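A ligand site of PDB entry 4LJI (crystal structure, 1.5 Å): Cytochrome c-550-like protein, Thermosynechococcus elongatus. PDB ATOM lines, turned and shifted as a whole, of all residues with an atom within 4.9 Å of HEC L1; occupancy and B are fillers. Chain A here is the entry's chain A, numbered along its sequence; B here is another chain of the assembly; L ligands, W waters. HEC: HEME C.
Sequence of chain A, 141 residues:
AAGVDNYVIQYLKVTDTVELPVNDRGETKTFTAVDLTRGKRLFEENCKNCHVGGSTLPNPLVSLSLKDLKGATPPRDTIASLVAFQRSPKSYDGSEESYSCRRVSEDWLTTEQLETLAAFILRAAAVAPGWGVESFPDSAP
SG of Cys 50 of chain B is bonded to CAC of HEC L2 (1.9 Å).
The side-chain hydroxyl (OG) of Ser 98 is in hydrogen-bond range of an oxygen (O2D) of HEC L1 (3.3 Å).
O2A of HEC L1 lies close to O of Ser 63.
An iron atom (FE) of HEC L1 is bound by the side-chain sulfur (SG) of Cys 101 (2.2 Å).
The side-chain sulfur (SG) of Cys 50 of chain A is covalently linked to a carbon (CAC) of HEC L1, at 1.9 Å.
An iron atom (FE) of HEC L1 is bound by a ring nitrogen (NE2) of His 51 (2.1 Å).
The side-chain sulfur (SG) of Cys 47 is covalently linked to a carbon (CAB) of HEC L1.
The guanidinium group (NH1) of Arg 76 is in salt-bridge range of an oxygen (O1A) of HEC L1, 2.9 Å away.
The backbone NH of Arg 76 is in hydrogen-bond range of the backbone carbonyl oxygen of Leu 69.
NH2 of Arg 76 is in hydrogen-bond range of O of Ser 91, 2.9 Å away.
The side-chain amide nitrogen of Gln 86 is in hydrogen-bond range of the backbone carbonyl oxygen of Arg 102, 2.8 Å away.
The backbone carbonyl oxygen of Asn 46 lies close to the side-chain amide nitrogen of Asn 49 of chain B, at 3.5 Å.
The side-chain hydroxyl of Tyr 92 lies within hydrogen-bond range of the backbone NH of Ala 72 (3.5 Å).
A ring nitrogen (ND1) of His 51 sits close to the side-chain hydroxyl (OG1) of Thr 56, at 3.1 Å.
The backbone carbonyl oxygen (O) of Val 62 lies within hydrogen-bond range of the side-chain hydroxyl (OG1) of Thr 56, at 2.6 Å.
The backbone carbonyl oxygen of Asp 68 is in hydrogen-bond range of the side-chain hydroxyl of Tyr 92, at 2.6 Å.
Asn 46 touches HEC L1.
Thr 56 touches HEC L1.
Val 62 touches HEC L1 (CG1 to CGA, 3.3 Å).
Leu 64 touches HEC L1 (CD2 to C3A, 3.5 Å).
CB of Asp 68 touches O2A of HEC L1 (3.4 Å).
N of Leu 69 touches O2A of HEC L1 (3.7 Å).
Ala 72 touches HEC L1.
Leu 82 touches HEC L1.
CE2 of Phe 85 touches C2A of HEC L1, 3.3 Å away.
Gln 86 touches HEC L1 (OE1 to CHB, 3.2 Å).
O of Lys 90 touches O2D of HEC L1, at 3.96 Å.
Tyr 92 touches HEC L1.
O of Ser 100 touches CHD of HEC L1, 3.2 Å away.
CB of Arg 102 touches CHC of HEC L1 (3.5 Å).
Val 104 touches HEC L1 (CG2 to CBB, 3.9 Å).
Leu 117 touches HEC L1.
Ile 121 touches HEC L1.
Asn 49 of chain B touches HEC L1.
Cys 50 of chain B touches HEC L1 (SG to CBC, 3.9 Å).
Hydrophobic or aromatic side chains within 4 Å of HEC L1: His 51, Val 62, Leu 64, Leu 69, Ala 72, Leu 82, Phe 85, Tyr 92, Val 104, Leu 117 and Ile 121.
26 residues have an atom within 4 Å of HEC L1: Asn 46, Cys 47, Cys 50 of chain A, His 51, Thr 56, Val 62, Ser 63, Leu 64, Asp 68, Leu 69, Ala 72, Arg 76, Leu 82, Phe 85, Gln 86, Lys 90, Tyr 92, Ser 98, Ser 100, Cys 101, Arg 102, Val 104, Leu 117, Ile 121, Asn 49 of chain B and Cys 50 of chain B.
Along chain A the residues within 4 Å of HEC L1 span positions 46 to 121.
Water W2 bridges O1D of HEC L1 (2.5 Å) and N of Tyr 92 (2.7 Å).
Water W1 lies within hydrogen-bond range of an oxygen (O1D) of HEC L1 (2.8 Å), the backbone carbonyl oxygen of Lys 90 (2.8 Å), the guanidinium group of Arg 76 (2.9 Å) and the backbone NH of Tyr 92 (3.2 Å).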
ATOM      1  N   ASN A  46      -8.384 -28.943  -0.055  1.00  0.00           N
ATOM      2  CA  ASN A  46      -8.551 -27.780  -0.904  1.00  0.00           C
ATOM      3  C   ASN A  46      -7.281 -27.085  -1.347  1.00  0.00           C
ATOM      4  O   ASN A  46      -7.324 -26.253  -2.261  1.00  0.00           O
ATOM      5  CB  ASN A  46      -9.453 -26.739  -0.215  1.00  0.00           C
ATOM      6  CG  ASN A  46     -10.860 -27.236  -0.032  1.00  0.00           C
ATOM      7  OD1 ASN A  46     -11.587 -27.415  -1.014  1.00  0.00           O
ATOM      8  ND2 ASN A  46     -11.244 -27.508   1.224  1.00  0.00           N
ATOM      9  N   CYS A  47      -6.178 -27.365  -0.646  1.00  0.00           N
ATOM     10  CA  CYS A  47      -4.989 -26.526  -0.774  1.00  0.00           C
ATOM     11  C   CYS A  47      -3.708 -27.302  -1.033  1.00  0.00           C
ATOM     12  O   CYS A  47      -2.672 -26.720  -1.382  1.00  0.00           O
ATOM     13  CB  CYS A  47      -4.786 -25.652   0.496  1.00  0.00           C
ATOM     14  SG  CYS A  47      -6.292 -24.903   1.091  1.00  0.00           S
ATOM     15  N   CYS A  50      -0.922 -27.382  -4.096  1.00  0.00           N
ATOM     16  CA  CYS A  50       0.030 -26.294  -4.249  1.00  0.00           C
ATOM     17  C   CYS A  50       0.857 -26.010  -3.022  1.00  0.00           C
ATOM     18  O   CYS A  50       1.918 -25.388  -3.098  1.00  0.00           O
ATOM     19  CB  CYS A  50      -0.696 -25.011  -4.720  1.00  0.00           C
ATOM     20  SG  CYS A  50      -1.459 -25.250  -6.392  1.00  0.00           S
ATOM     21  N   HIS A  51       0.335 -26.425  -1.866  1.00  0.00           N
ATOM     22  CA  HIS A  51       0.923 -25.923  -0.605  1.00  0.00           C
ATOM     23  C   HIS A  51       1.337 -27.057   0.289  1.00  0.00           C
ATOM     24  O   HIS A  51       1.506 -26.881   1.499  1.00  0.00           O
ATOM     25  CB  HIS A  51      -0.043 -25.015   0.158  1.00  0.00           C
ATOM     26  CG  HIS A  51      -0.264 -23.693  -0.485  1.00  0.00           C
ATOM     27  ND1 HIS A  51       0.749 -22.775  -0.653  1.00  0.00           N
ATOM     28  CD2 HIS A  51      -1.394 -23.096  -0.932  1.00  0.00           C
ATOM     29  CE1 HIS A  51       0.246 -21.665  -1.188  1.00  0.00           C
ATOM     30  NE2 HIS A  51      -1.033 -21.863  -1.388  1.00  0.00           N
ATOM     31  N   THR A  56       4.951 -23.371  -1.471  1.00  0.00           N
ATOM     32  CA  THR A  56       4.081 -22.884  -2.525  1.00  0.00           C
ATOM     33  C   THR A  56       4.670 -23.315  -3.851  1.00  0.00           C
ATOM     34  O   THR A  56       5.586 -22.683  -4.332  1.00  0.00           O
ATOM     35  CB  THR A  56       3.908 -21.349  -2.458  1.00  0.00           C
ATOM     36  OG1 THR A  56       3.262 -21.013  -1.216  1.00  0.00           O
ATOM     37  CG2 THR A  56       3.022 -20.828  -3.598  1.00  0.00           C
ATOM     38  N   PRO A  58       3.827 -23.308  -7.119  1.00  0.00           N
ATOM     39  CA  PRO A  58       3.942 -22.435  -8.290  1.00  0.00           C
ATOM     40  C   PRO A  58       4.676 -21.108  -8.065  1.00  0.00           C
ATOM     41  O   PRO A  58       4.997 -20.424  -9.035  1.00  0.00           O
ATOM     42  CB  PRO A  58       2.493 -22.181  -8.692  1.00  0.00           C
ATOM     43  CG  PRO A  58       1.717 -23.245  -8.044  1.00  0.00           C
ATOM     44  CD  PRO A  58       2.414 -23.495  -6.748  1.00  0.00           C
ATOM     45  N   ASN A  59       4.917 -20.728  -6.812  1.00  0.00           N
ATOM     46  CA  ASN A  59       5.794 -19.604  -6.524  1.00  0.00           C
ATOM     47  C   ASN A  59       6.464 -19.807  -5.173  1.00  0.00           C
ATOM     48  O   ASN A  59       5.971 -19.315  -4.166  1.00  0.00           O
ATOM     49  CB  ASN A  59       5.031 -18.262  -6.530  1.00  0.00           C
ATOM     50  CG  ASN A  59       5.947 -17.073  -6.233  1.00  0.00           C
ATOM     51  OD1 ASN A  59       7.173 -17.177  -6.312  1.00  0.00           O
ATOM     52  ND2 ASN A  59       5.348 -15.928  -5.916  1.00  0.00           N
ATOM     53  N   VAL A  62       6.898 -17.196  -2.254  1.00  0.00           N
ATOM     54  CA  VAL A  62       5.762 -16.791  -1.408  1.00  0.00           C
ATOM     55  C   VAL A  62       5.127 -18.041  -0.763  1.00  0.00           C
ATOM     56  O   VAL A  62       4.027 -18.483  -1.148  1.00  0.00           O
ATOM     57  CB  VAL A  62       4.714 -15.930  -2.205  1.00  0.00           C
ATOM     58  CG1 VAL A  62       3.547 -15.491  -1.310  1.00  0.00           C
ATOM     59  CG2 VAL A  62       5.393 -14.728  -2.849  1.00  0.00           C
ATOM     60  N   SER A  63       5.826 -18.607   0.232  1.00  0.00           N
ATOM     61  CA  SER A  63       5.411 -19.849   0.867  1.00  0.00           C
ATOM     62  C   SER A  63       4.464 -19.601   2.055  1.00  0.00           C
ATOM     63  O   SER A  63       4.093 -18.438   2.319  1.00  0.00           O
ATOM     64  CB  SER A  63       6.631 -20.625   1.363  1.00  0.00           C
ATOM     65  OG  SER A  63       7.135 -20.058   2.552  1.00  0.00           O
ATOM     66  N   LEU A  64       4.094 -20.669   2.757  1.00  0.00           N
ATOM     67  CA  LEU A  64       3.280 -20.535   3.966  1.00  0.00           C
ATOM     68  C   LEU A  64       4.131 -20.506   5.220  1.00  0.00           C
ATOM     69  O   LEU A  64       3.630 -20.716   6.336  1.00  0.00           O
ATOM     70  CB  LEU A  64       2.146 -21.580   4.039  1.00  0.00           C
ATOM     71  CG  LEU A  64       1.277 -21.689   2.790  1.00  0.00           C
ATOM     72  CD1 LEU A  64       0.145 -22.716   3.004  1.00  0.00           C
ATOM     73  CD2 LEU A  64       0.749 -20.332   2.307  1.00  0.00           C
ATOM     74  N   ASP A  68       7.370 -15.751   5.580  1.00  0.00           N
ATOM     75  CA  ASP A  68       6.770 -15.257   4.345  1.00  0.00           C
ATOM     76  C   ASP A  68       5.386 -14.639   4.651  1.00  0.00           C
ATOM     77  O   ASP A  68       5.053 -13.567   4.161  1.00  0.00           O
ATOM     78  CB  ASP A  68       6.672 -16.371   3.310  1.00  0.00           C
ATOM     79  CG  ASP A  68       8.042 -16.703   2.684  1.00  0.00           C
ATOM     80  OD1 ASP A  68       9.047 -16.000   2.982  1.00  0.00           O
ATOM     81  OD2 ASP A  68       8.112 -17.628   1.852  1.00  0.00           O
ATOM     82  N   LEU A  69       4.641 -15.295   5.517  1.00  0.00           N
ATOM     83  CA  LEU A  69       3.360 -14.743   5.951  1.00  0.00           C
ATOM     84  C   LEU A  69       3.514 -13.385   6.595  1.00  0.00           C
ATOM     85  O   LEU A  69       2.773 -12.448   6.270  1.00  0.00           O
ATOM     86  CB  LEU A  69       2.650 -15.700   6.909  1.00  0.00           C
ATOM     87  CG  LEU A  69       2.167 -17.006   6.247  1.00  0.00           C
ATOM     88  CD1 LEU A  69       1.717 -17.990   7.331  1.00  0.00           C
ATOM     89  CD2 LEU A  69       1.051 -16.723   5.214  1.00  0.00           C
ATOM     90  N   ALA A  72       4.164 -10.330   4.202  1.00  0.00           N
ATOM     91  CA  ALA A  72       3.156  -9.904   3.242  1.00  0.00           C
ATOM     92  C   ALA A  72       2.606  -8.531   3.616  1.00  0.00           C
ATOM     93  O   ALA A  72       2.820  -8.070   4.731  1.00  0.00           O
ATOM     94  CB  ALA A  72       2.036 -10.929   3.157  1.00  0.00           C
ATOM     95  N   ARG A  76       0.221 -11.569   6.971  1.00  0.00           N
ATOM     96  CA  ARG A  76      -0.763 -12.645   6.898  1.00  0.00           C
ATOM     97  C   ARG A  76      -0.545 -13.611   8.053  1.00  0.00           C
ATOM     98  O   ARG A  76      -0.459 -14.841   7.889  1.00  0.00           O
ATOM     99  CB  ARG A  76      -0.664 -13.320   5.520  1.00  0.00           C
ATOM    100  CG  ARG A  76      -1.035 -12.327   4.440  1.00  0.00           C
ATOM    101  CD  ARG A  76      -0.909 -12.858   3.039  1.00  0.00           C
ATOM    102  NE  ARG A  76      -1.198 -11.802   2.059  1.00  0.00           N
ATOM    103  CZ  ARG A  76      -0.717 -11.761   0.818  1.00  0.00           C
ATOM    104  NH1 ARG A  76       0.116 -12.697   0.416  1.00  0.00           N
ATOM    105  NH2 ARG A  76      -1.047 -10.754   0.005  1.00  0.00           N
ATOM    106  N   LEU A  82      -5.704 -13.818   7.273  1.00  0.00           N
ATOM    107  CA  LEU A  82      -5.659 -15.026   6.393  1.00  0.00           C
ATOM    108  C   LEU A  82      -7.054 -15.236   5.780  1.00  0.00           C
ATOM    109  O   LEU A  82      -7.177 -15.575   4.613  1.00  0.00           O
ATOM    110  CB  LEU A  82      -5.198 -16.266   7.156  1.00  0.00           C
ATOM    111  CG  LEU A  82      -3.700 -16.279   7.415  1.00  0.00           C
ATOM    112  CD1 LEU A  82      -3.380 -17.355   8.431  1.00  0.00           C
ATOM    113  CD2 LEU A  82      -3.027 -16.546   6.120  1.00  0.00           C
ATOM    114  N   PHE A  85      -7.605 -12.832   3.066  1.00  0.00           N
ATOM    115  CA  PHE A  85      -6.759 -13.173   1.931  1.00  0.00           C
ATOM    116  C   PHE A  85      -7.484 -14.217   1.108  1.00  0.00           C
ATOM    117  O   PHE A  85      -7.617 -14.088  -0.105  1.00  0.00           O
ATOM    118  CB  PHE A  85      -5.384 -13.703   2.350  1.00  0.00           C
ATOM    119  CG  PHE A  85      -4.564 -14.169   1.215  1.00  0.00           C
ATOM    120  CD1 PHE A  85      -3.862 -13.249   0.429  1.00  0.00           C
ATOM    121  CD2 PHE A  85      -4.542 -15.509   0.889  1.00  0.00           C
ATOM    122  CE1 PHE A  85      -3.127 -13.699  -0.668  1.00  0.00           C
ATOM    123  CE2 PHE A  85      -3.807 -15.979  -0.186  1.00  0.00           C
ATOM    124  CZ  PHE A  85      -3.087 -15.043  -0.967  1.00  0.00           C
ATOM    125  N   GLN A  86      -8.009 -15.221   1.785  1.00  0.00           N
ATOM    126  CA  GLN A  86      -8.593 -16.342   1.054  1.00  0.00           C
ATOM    127  C   GLN A  86      -9.870 -15.941   0.325  1.00  0.00           C
ATOM    128  O   GLN A  86     -10.225 -16.527  -0.699  1.00  0.00           O
ATOM    129  CB  GLN A  86      -8.796 -17.548   1.948  1.00  0.00           C
ATOM    130  CG  GLN A  86      -8.362 -18.817   1.176  1.00  0.00           C
ATOM    131  CD  GLN A  86      -6.931 -18.743   0.739  1.00  0.00           C
ATOM    132  OE1 GLN A  86      -6.060 -18.420   1.530  1.00  0.00           O
ATOM    133  NE2 GLN A  86      -6.659 -19.032  -0.532  1.00  0.00           N
ATOM    134  N   LYS A  90      -4.535 -11.700  -2.957  1.00  0.00           N
ATOM    135  CA  LYS A  90      -3.832 -10.549  -3.472  1.00  0.00           C
ATOM    136  C   LYS A  90      -2.369 -10.879  -3.776  1.00  0.00           C
ATOM    137  O   LYS A  90      -1.845 -11.935  -3.372  1.00  0.00           O
ATOM    138  CB  LYS A  90      -3.877  -9.408  -2.447  1.00  0.00           C
ATOM    139  CG  LYS A  90      -5.281  -8.876  -2.071  1.00  0.00           C
ATOM    140  CD  LYS A  90      -5.841  -7.997  -3.180  1.00  0.00           C
ATOM    141  CE  LYS A  90      -7.248  -7.552  -2.814  1.00  0.00           C
ATOM    142  NZ  LYS A  90      -8.176  -8.689  -3.042  1.00  0.00           N
ATOM    143  N   SER A  91      -1.685  -9.951  -4.455  1.00  0.00           N
ATOM    144  CA  SER A  91      -0.250 -10.108  -4.661  1.00  0.00           C
ATOM    145  C   SER A  91       0.498  -9.930  -3.340  1.00  0.00           C
ATOM    146  O   SER A  91      -0.060  -9.428  -2.359  1.00  0.00           O
ATOM    147  CB  SER A  91       0.280  -9.140  -5.733  1.00  0.00           C
ATOM    148  OG  SER A  91       0.075  -7.804  -5.363  1.00  0.00           O
ATOM    149  N   TYR A  92       1.768 -10.341  -3.305  1.00  0.00           N
ATOM    150  CA  TYR A  92       2.522 -10.289  -2.048  1.00  0.00           C
ATOM    151  C   TYR A  92       2.660  -8.886  -1.434  1.00  0.00           C
ATOM    152  O   TYR A  92       2.680  -8.757  -0.230  1.00  0.00           O
ATOM    153  CB  TYR A  92       3.897 -10.927  -2.219  1.00  0.00           C
ATOM    154  CG  TYR A  92       4.615 -11.243  -0.934  1.00  0.00           C
ATOM    155  CD1 TYR A  92       4.131 -12.205  -0.062  1.00  0.00           C
ATOM    156  CD2 TYR A  92       5.797 -10.597  -0.577  1.00  0.00           C
ATOM    157  CE1 TYR A  92       4.788 -12.514   1.104  1.00  0.00           C
ATOM    158  CE2 TYR A  92       6.456 -10.896   0.582  1.00  0.00           C
ATOM    159  CZ  TYR A  92       5.961 -11.873   1.412  1.00  0.00           C
ATOM    160  OH  TYR A  92       6.617 -12.182   2.579  1.00  0.00           O
ATOM    161  N   SER A  98      -4.520 -11.399  -7.106  1.00  0.00           N
ATOM    162  CA  SER A  98      -3.883 -12.624  -7.612  1.00  0.00           C
ATOM    163  C   SER A  98      -4.897 -13.692  -8.031  1.00  0.00           C
ATOM    164  O   SER A  98      -5.873 -13.977  -7.332  1.00  0.00           O
ATOM    165  CB  SER A  98      -2.903 -13.203  -6.579  1.00  0.00           C
ATOM    166  OG  SER A  98      -2.548 -14.543  -6.926  1.00  0.00           O
ATOM    167  N   SER A 100      -3.574 -16.658  -8.975  1.00  0.00           N
ATOM    168  CA  SER A 100      -2.671 -17.827  -8.928  1.00  0.00           C
ATOM    169  C   SER A 100      -2.944 -18.760  -7.734  1.00  0.00           C
ATOM    170  O   SER A 100      -2.508 -19.912  -7.711  1.00  0.00           O
ATOM    171  CB  SER A 100      -1.226 -17.360  -8.870  1.00  0.00           C
ATOM    172  OG  SER A 100      -0.915 -16.527  -9.975  1.00  0.00           O
ATOM    173  N   CYS A 101      -3.613 -18.230  -6.722  1.00  0.00           N
ATOM    174  CA  CYS A 101      -4.005 -19.002  -5.552  1.00  0.00           C
ATOM    175  C   CYS A 101      -5.500 -19.311  -5.723  1.00  0.00           C
ATOM    176  O   CYS A 101      -6.086 -18.962  -6.739  1.00  0.00           O
ATOM    177  CB  CYS A 101      -3.713 -18.194  -4.260  1.00  0.00           C
ATOM    178  SG  CYS A 101      -3.991 -18.963  -2.614  1.00  0.00           S
ATOM    179  N   ARG A 102      -6.106 -19.960  -4.736  1.00  0.00           N
ATOM    180  CA  ARG A 102      -7.484 -20.459  -4.838  1.00  0.00           C
ATOM    181  C   ARG A 102      -8.389 -19.551  -4.035  1.00  0.00           C
ATOM    182  O   ARG A 102      -8.304 -19.505  -2.808  1.00  0.00           O
ATOM    183  CB  ARG A 102      -7.567 -21.893  -4.283  1.00  0.00           C
ATOM    184  CG  ARG A 102      -8.934 -22.513  -4.351  1.00  0.00           C
ATOM    185  CD  ARG A 102      -9.539 -22.332  -5.718  1.00  0.00           C
ATOM    186  NE  ARG A 102     -10.666 -23.238  -5.915  1.00  0.00           N
ATOM    187  CZ  ARG A 102     -10.561 -24.435  -6.472  1.00  0.00           C
ATOM    188  NH1 ARG A 102     -11.638 -25.207  -6.593  1.00  0.00           N
ATOM    189  NH2 ARG A 102      -9.380 -24.862  -6.908  1.00  0.00           N
ATOM    190  N   VAL A 104     -11.701 -18.533  -2.198  1.00  0.00           N
ATOM    191  CA  VAL A 104     -12.673 -19.377  -1.561  1.00  0.00           C
ATOM    192  C   VAL A 104     -13.920 -18.535  -1.258  1.00  0.00           C
ATOM    193  O   VAL A 104     -13.884 -17.638  -0.422  1.00  0.00           O
ATOM    194  CB  VAL A 104     -12.137 -20.015  -0.294  1.00  0.00           C
ATOM    195  CG1 VAL A 104     -13.205 -20.836   0.373  1.00  0.00           C
ATOM    196  CG2 VAL A 104     -10.957 -20.932  -0.633  1.00  0.00           C
ATOM    197  N   LEU A 117      -9.280 -23.200   9.001  1.00  0.00           N
ATOM    198  CA  LEU A 117      -8.204 -23.420   8.013  1.00  0.00           C
ATOM    199  C   LEU A 117      -7.094 -22.401   8.275  1.00  0.00           C
ATOM    200  O   LEU A 117      -5.906 -22.744   8.295  1.00  0.00           O
ATOM    201  CB  LEU A 117      -8.757 -23.340   6.585  1.00  0.00           C
ATOM    202  CG  LEU A 117      -7.846 -23.296   5.356  1.00  0.00           C
ATOM    203  CD1 LEU A 117      -6.915 -24.510   5.376  1.00  0.00           C
ATOM    204  CD2 LEU A 117      -8.707 -23.320   4.080  1.00  0.00           C
ATOM    205  N   ILE A 121      -3.149 -23.243   9.394  1.00  0.00           N
ATOM    206  CA  ILE A 121      -1.986 -22.730   8.682  1.00  0.00           C
ATOM    207  C   ILE A 121      -1.126 -21.942   9.654  1.00  0.00           C
ATOM    208  O   ILE A 121       0.105 -22.072   9.654  1.00  0.00           O
ATOM    209  CB  ILE A 121      -2.392 -21.804   7.515  1.00  0.00           C
ATOM    210  CG1 ILE A 121      -3.036 -22.624   6.387  1.00  0.00           C
ATOM    211  CG2 ILE A 121      -1.166 -21.044   6.958  1.00  0.00           C
ATOM    212  CD1 ILE A 121      -3.696 -21.743   5.354  1.00  0.00           C
ATOM    213  N   ASN B  49      -7.256 -29.927  -6.852  1.00  0.00           N
ATOM    214  CA  ASN B  49      -7.470 -28.502  -6.564  1.00  0.00           C
ATOM    215  C   ASN B  49      -7.556 -27.754  -7.912  1.00  0.00           C
ATOM    216  O   ASN B  49      -8.205 -26.715  -8.012  1.00  0.00           O
ATOM    217  CB  ASN B  49      -6.306 -27.865  -5.781  1.00  0.00           C
ATOM    218  CG  ASN B  49      -5.992 -28.508  -4.413  1.00  0.00           C
ATOM    219  OD1 ASN B  49      -4.926 -28.219  -3.918  1.00  0.00           O
ATOM    220  ND2 ASN B  49      -6.867 -29.343  -3.823  1.00  0.00           N
ATOM    221  N   CYS B  50      -6.830 -28.275  -8.913  1.00  0.00           N
ATOM    222  CA  CYS B  50      -6.891 -27.719 -10.258  1.00  0.00           C
ATOM    223  C   CYS B  50      -7.854 -28.474 -11.150  1.00  0.00           C
ATOM    224  O   CYS B  50      -8.286 -27.928 -12.147  1.00  0.00           O
ATOM    225  CB  CYS B  50      -5.497 -27.760 -10.929  1.00  0.00           C
ATOM    226  SG  CYS B  50      -4.337 -26.649 -10.064  1.00  0.00           S
HETATM  227 FE   HEC L   1      -2.416 -20.422  -2.068  1.00  0.00          FE
HETATM  228  CHA HEC L   1      -0.263 -17.733  -1.795  1.00  0.00           C
HETATM  229  CHB HEC L   1      -3.345 -20.040   1.238  1.00  0.00           C
HETATM  230  CHC HEC L   1      -4.834 -22.947  -2.410  1.00  0.00           C
HETATM  231  CHD HEC L   1      -1.202 -21.164  -5.118  1.00  0.00           C
HETATM  232  NA  HEC L   1      -1.886 -19.203  -0.567  1.00  0.00           N
HETATM  233  C1A HEC L   1      -1.010 -18.128  -0.695  1.00  0.00           C
HETATM  234  C2A HEC L   1      -0.917 -17.468   0.592  1.00  0.00           C
HETATM  235  C3A HEC L   1      -1.769 -18.119   1.419  1.00  0.00           C
HETATM  236  C4A HEC L   1      -2.406 -19.160   0.728  1.00  0.00           C
HETATM  237  CMA HEC L   1      -2.050 -17.772   2.857  1.00  0.00           C
HETATM  238  CAA HEC L   1      -0.027 -16.274   0.960  1.00  0.00           C
HETATM  239  CBA HEC L   1       1.385 -16.740   1.360  1.00  0.00           C
HETATM  240  CGA HEC L   1       2.316 -15.626   1.759  1.00  0.00           C
HETATM  241  O1A HEC L   1       1.934 -14.431   1.860  1.00  0.00           O
HETATM  242  O2A HEC L   1       3.536 -15.906   2.023  1.00  0.00           O
HETATM  243  NB  HEC L   1      -3.819 -21.348  -0.828  1.00  0.00           N
HETATM  244  C1B HEC L   1      -4.039 -20.989   0.451  1.00  0.00           C
HETATM  245  C2B HEC L   1      -5.058 -21.800   0.975  1.00  0.00           C
HETATM  246  C3B HEC L   1      -5.539 -22.615  -0.025  1.00  0.00           C
HETATM  247  C4B HEC L   1      -4.684 -22.313  -1.188  1.00  0.00           C
HETATM  248  CMB HEC L   1      -5.602 -21.707   2.381  1.00  0.00           C
HETATM  249  CAB HEC L   1      -6.613 -23.640   0.052  1.00  0.00           C
HETATM  250  CBB HEC L   1      -7.855 -23.064   0.255  1.00  0.00           C
HETATM  251  NC  HEC L   1      -2.925 -21.810  -3.497  1.00  0.00           N
HETATM  252  C1C HEC L   1      -3.949 -22.715  -3.443  1.00  0.00           C
HETATM  253  C2C HEC L   1      -3.845 -23.526  -4.580  1.00  0.00           C
HETATM  254  C3C HEC L   1      -2.832 -23.043  -5.363  1.00  0.00           C
HETATM  255  C4C HEC L   1      -2.240 -21.932  -4.680  1.00  0.00           C
HETATM  256  CMC HEC L   1      -4.748 -24.712  -4.892  1.00  0.00           C
HETATM  257  CAC HEC L   1      -2.377 -23.653  -6.646  1.00  0.00           C
HETATM  258  CBC HEC L   1      -3.201 -23.729  -7.714  1.00  0.00           C
HETATM  259  ND  HEC L   1      -1.016 -19.608  -3.202  1.00  0.00           N
HETATM  260  C1D HEC L   1      -0.720 -20.036  -4.432  1.00  0.00           C
HETATM  261  C2D HEC L   1       0.276 -19.141  -5.037  1.00  0.00           C
HETATM  262  C3D HEC L   1       0.561 -18.193  -4.121  1.00  0.00           C
HETATM  263  C4D HEC L   1      -0.259 -18.514  -2.958  1.00  0.00           C
HETATM  264  CMD HEC L   1       0.875 -19.288  -6.421  1.00  0.00           C
HETATM  265  CAD HEC L   1       1.498 -17.037  -4.298  1.00  0.00           C
HETATM  266  CBD HEC L   1       0.626 -15.806  -4.626  1.00  0.00           C
HETATM  267  CGD HEC L   1       1.132 -14.442  -5.059  1.00  0.00           C
HETATM  268  O1D HEC L   1       2.153 -13.894  -4.556  1.00  0.00           O
HETATM  269  O2D HEC L   1       0.486 -13.834  -5.945  1.00  0.00           O
HETATM  270 FE   HEC L   2      -2.951 -31.212 -14.639  1.00  0.00          FE
HETATM  271  CHA HEC L   2      -3.330 -30.704 -18.031  1.00  0.00           C
HETATM  272  CHB HEC L   2      -3.335 -34.559 -15.069  1.00  0.00           C
HETATM  273  CHC HEC L   2      -2.156 -31.746 -11.255  1.00  0.00           C
HETATM  274  CHD HEC L   2      -3.125 -27.882 -14.065  1.00  0.00           C
HETATM  275  NA  HEC L   2      -3.312 -32.411 -16.204  1.00  0.00           N
HETATM  276  C1A HEC L   2      -3.427 -31.986 -17.519  1.00  0.00           C
HETATM  277  C2A HEC L   2      -3.724 -33.133 -18.318  1.00  0.00           C
HETATM  278  C3A HEC L   2      -3.720 -34.235 -17.515  1.00  0.00           C
HETATM  279  C4A HEC L   2      -3.425 -33.782 -16.198  1.00  0.00           C
HETATM  280  CMA HEC L   2      -3.966 -35.674 -17.882  1.00  0.00           C
HETATM  281  CAA HEC L   2      -3.979 -33.139 -19.817  1.00  0.00           C
HETATM  282  CBA HEC L   2      -5.481 -33.098 -20.127  1.00  0.00           C
HETATM  283  CGA HEC L   2      -5.817 -33.150 -21.613  1.00  0.00           C
HETATM  284  O1A HEC L   2      -4.915 -33.418 -22.401  1.00  0.00           O
HETATM  285  O2A HEC L   2      -6.980 -32.964 -22.065  1.00  0.00           O
HETATM  286  NB  HEC L   2      -2.733 -32.837 -13.385  1.00  0.00           N
HETATM  287  C1B HEC L   2      -2.974 -34.087 -13.797  1.00  0.00           C
HETATM  288  C2B HEC L   2      -2.799 -34.974 -12.687  1.00  0.00           C
HETATM  289  C3B HEC L   2      -2.446 -34.227 -11.572  1.00  0.00           C
HETATM  290  C4B HEC L   2      -2.446 -32.849 -12.077  1.00  0.00           C
HETATM  291  CMB HEC L   2      -2.915 -36.485 -12.744  1.00  0.00           C
HETATM  292  CAB HEC L   2      -2.183 -34.706 -10.168  1.00  0.00           C
HETATM  293  CBB HEC L   2      -0.962 -35.298 -10.072  1.00  0.00           C
HETATM  294  NC  HEC L   2      -2.652 -30.050 -12.948  1.00  0.00           N
HETATM  295  C1C HEC L   2      -2.356 -30.450 -11.684  1.00  0.00           C
HETATM  296  C2C HEC L   2      -2.399 -29.307 -10.872  1.00  0.00           C
HETATM  297  C3C HEC L   2      -2.659 -28.213 -11.657  1.00  0.00           C
HETATM  298  C4C HEC L   2      -2.815 -28.685 -12.993  1.00  0.00           C
HETATM  299  CMC HEC L   2      -2.143 -29.353  -9.384  1.00  0.00           C
HETATM  300  CAC HEC L   2      -2.839 -26.810 -11.143  1.00  0.00           C
HETATM  301  CBC HEC L   2      -1.760 -26.111 -10.742  1.00  0.00           C
HETATM  302  ND  HEC L   2      -3.197 -29.646 -15.797  1.00  0.00           N
HETATM  303  C1D HEC L   2      -3.188 -28.365 -15.376  1.00  0.00           C
HETATM  304  C2D HEC L   2      -3.208 -27.427 -16.474  1.00  0.00           C
HETATM  305  C3D HEC L   2      -3.248 -28.200 -17.594  1.00  0.00           C
HETATM  306  C4D HEC L   2      -3.274 -29.598 -17.128  1.00  0.00           C
HETATM  307  CMD HEC L   2      -3.192 -25.927 -16.413  1.00  0.00           C
HETATM  308  CAD HEC L   2      -3.255 -27.713 -19.015  1.00  0.00           C
HETATM  309  CBD HEC L   2      -1.818 -28.017 -19.497  1.00  0.00           C
HETATM  310  CGD HEC L   2      -1.254 -27.499 -20.780  1.00  0.00           C
HETATM  311  O1D HEC L   2      -0.120 -26.957 -20.812  1.00  0.00           O
HETATM  312  O2D HEC L   2      -1.922 -27.619 -21.817  1.00  0.00           O
HETATM  313  O   HOH W   1       0.513 -13.126  -2.433  1.00  0.00           O
HETATM  314  O   HOH W   2       2.835 -11.692  -5.431  1.00  0.00           O
HETATM  315  O   HOH W   3       2.227 -15.938  -7.894  1.00  0.00           O
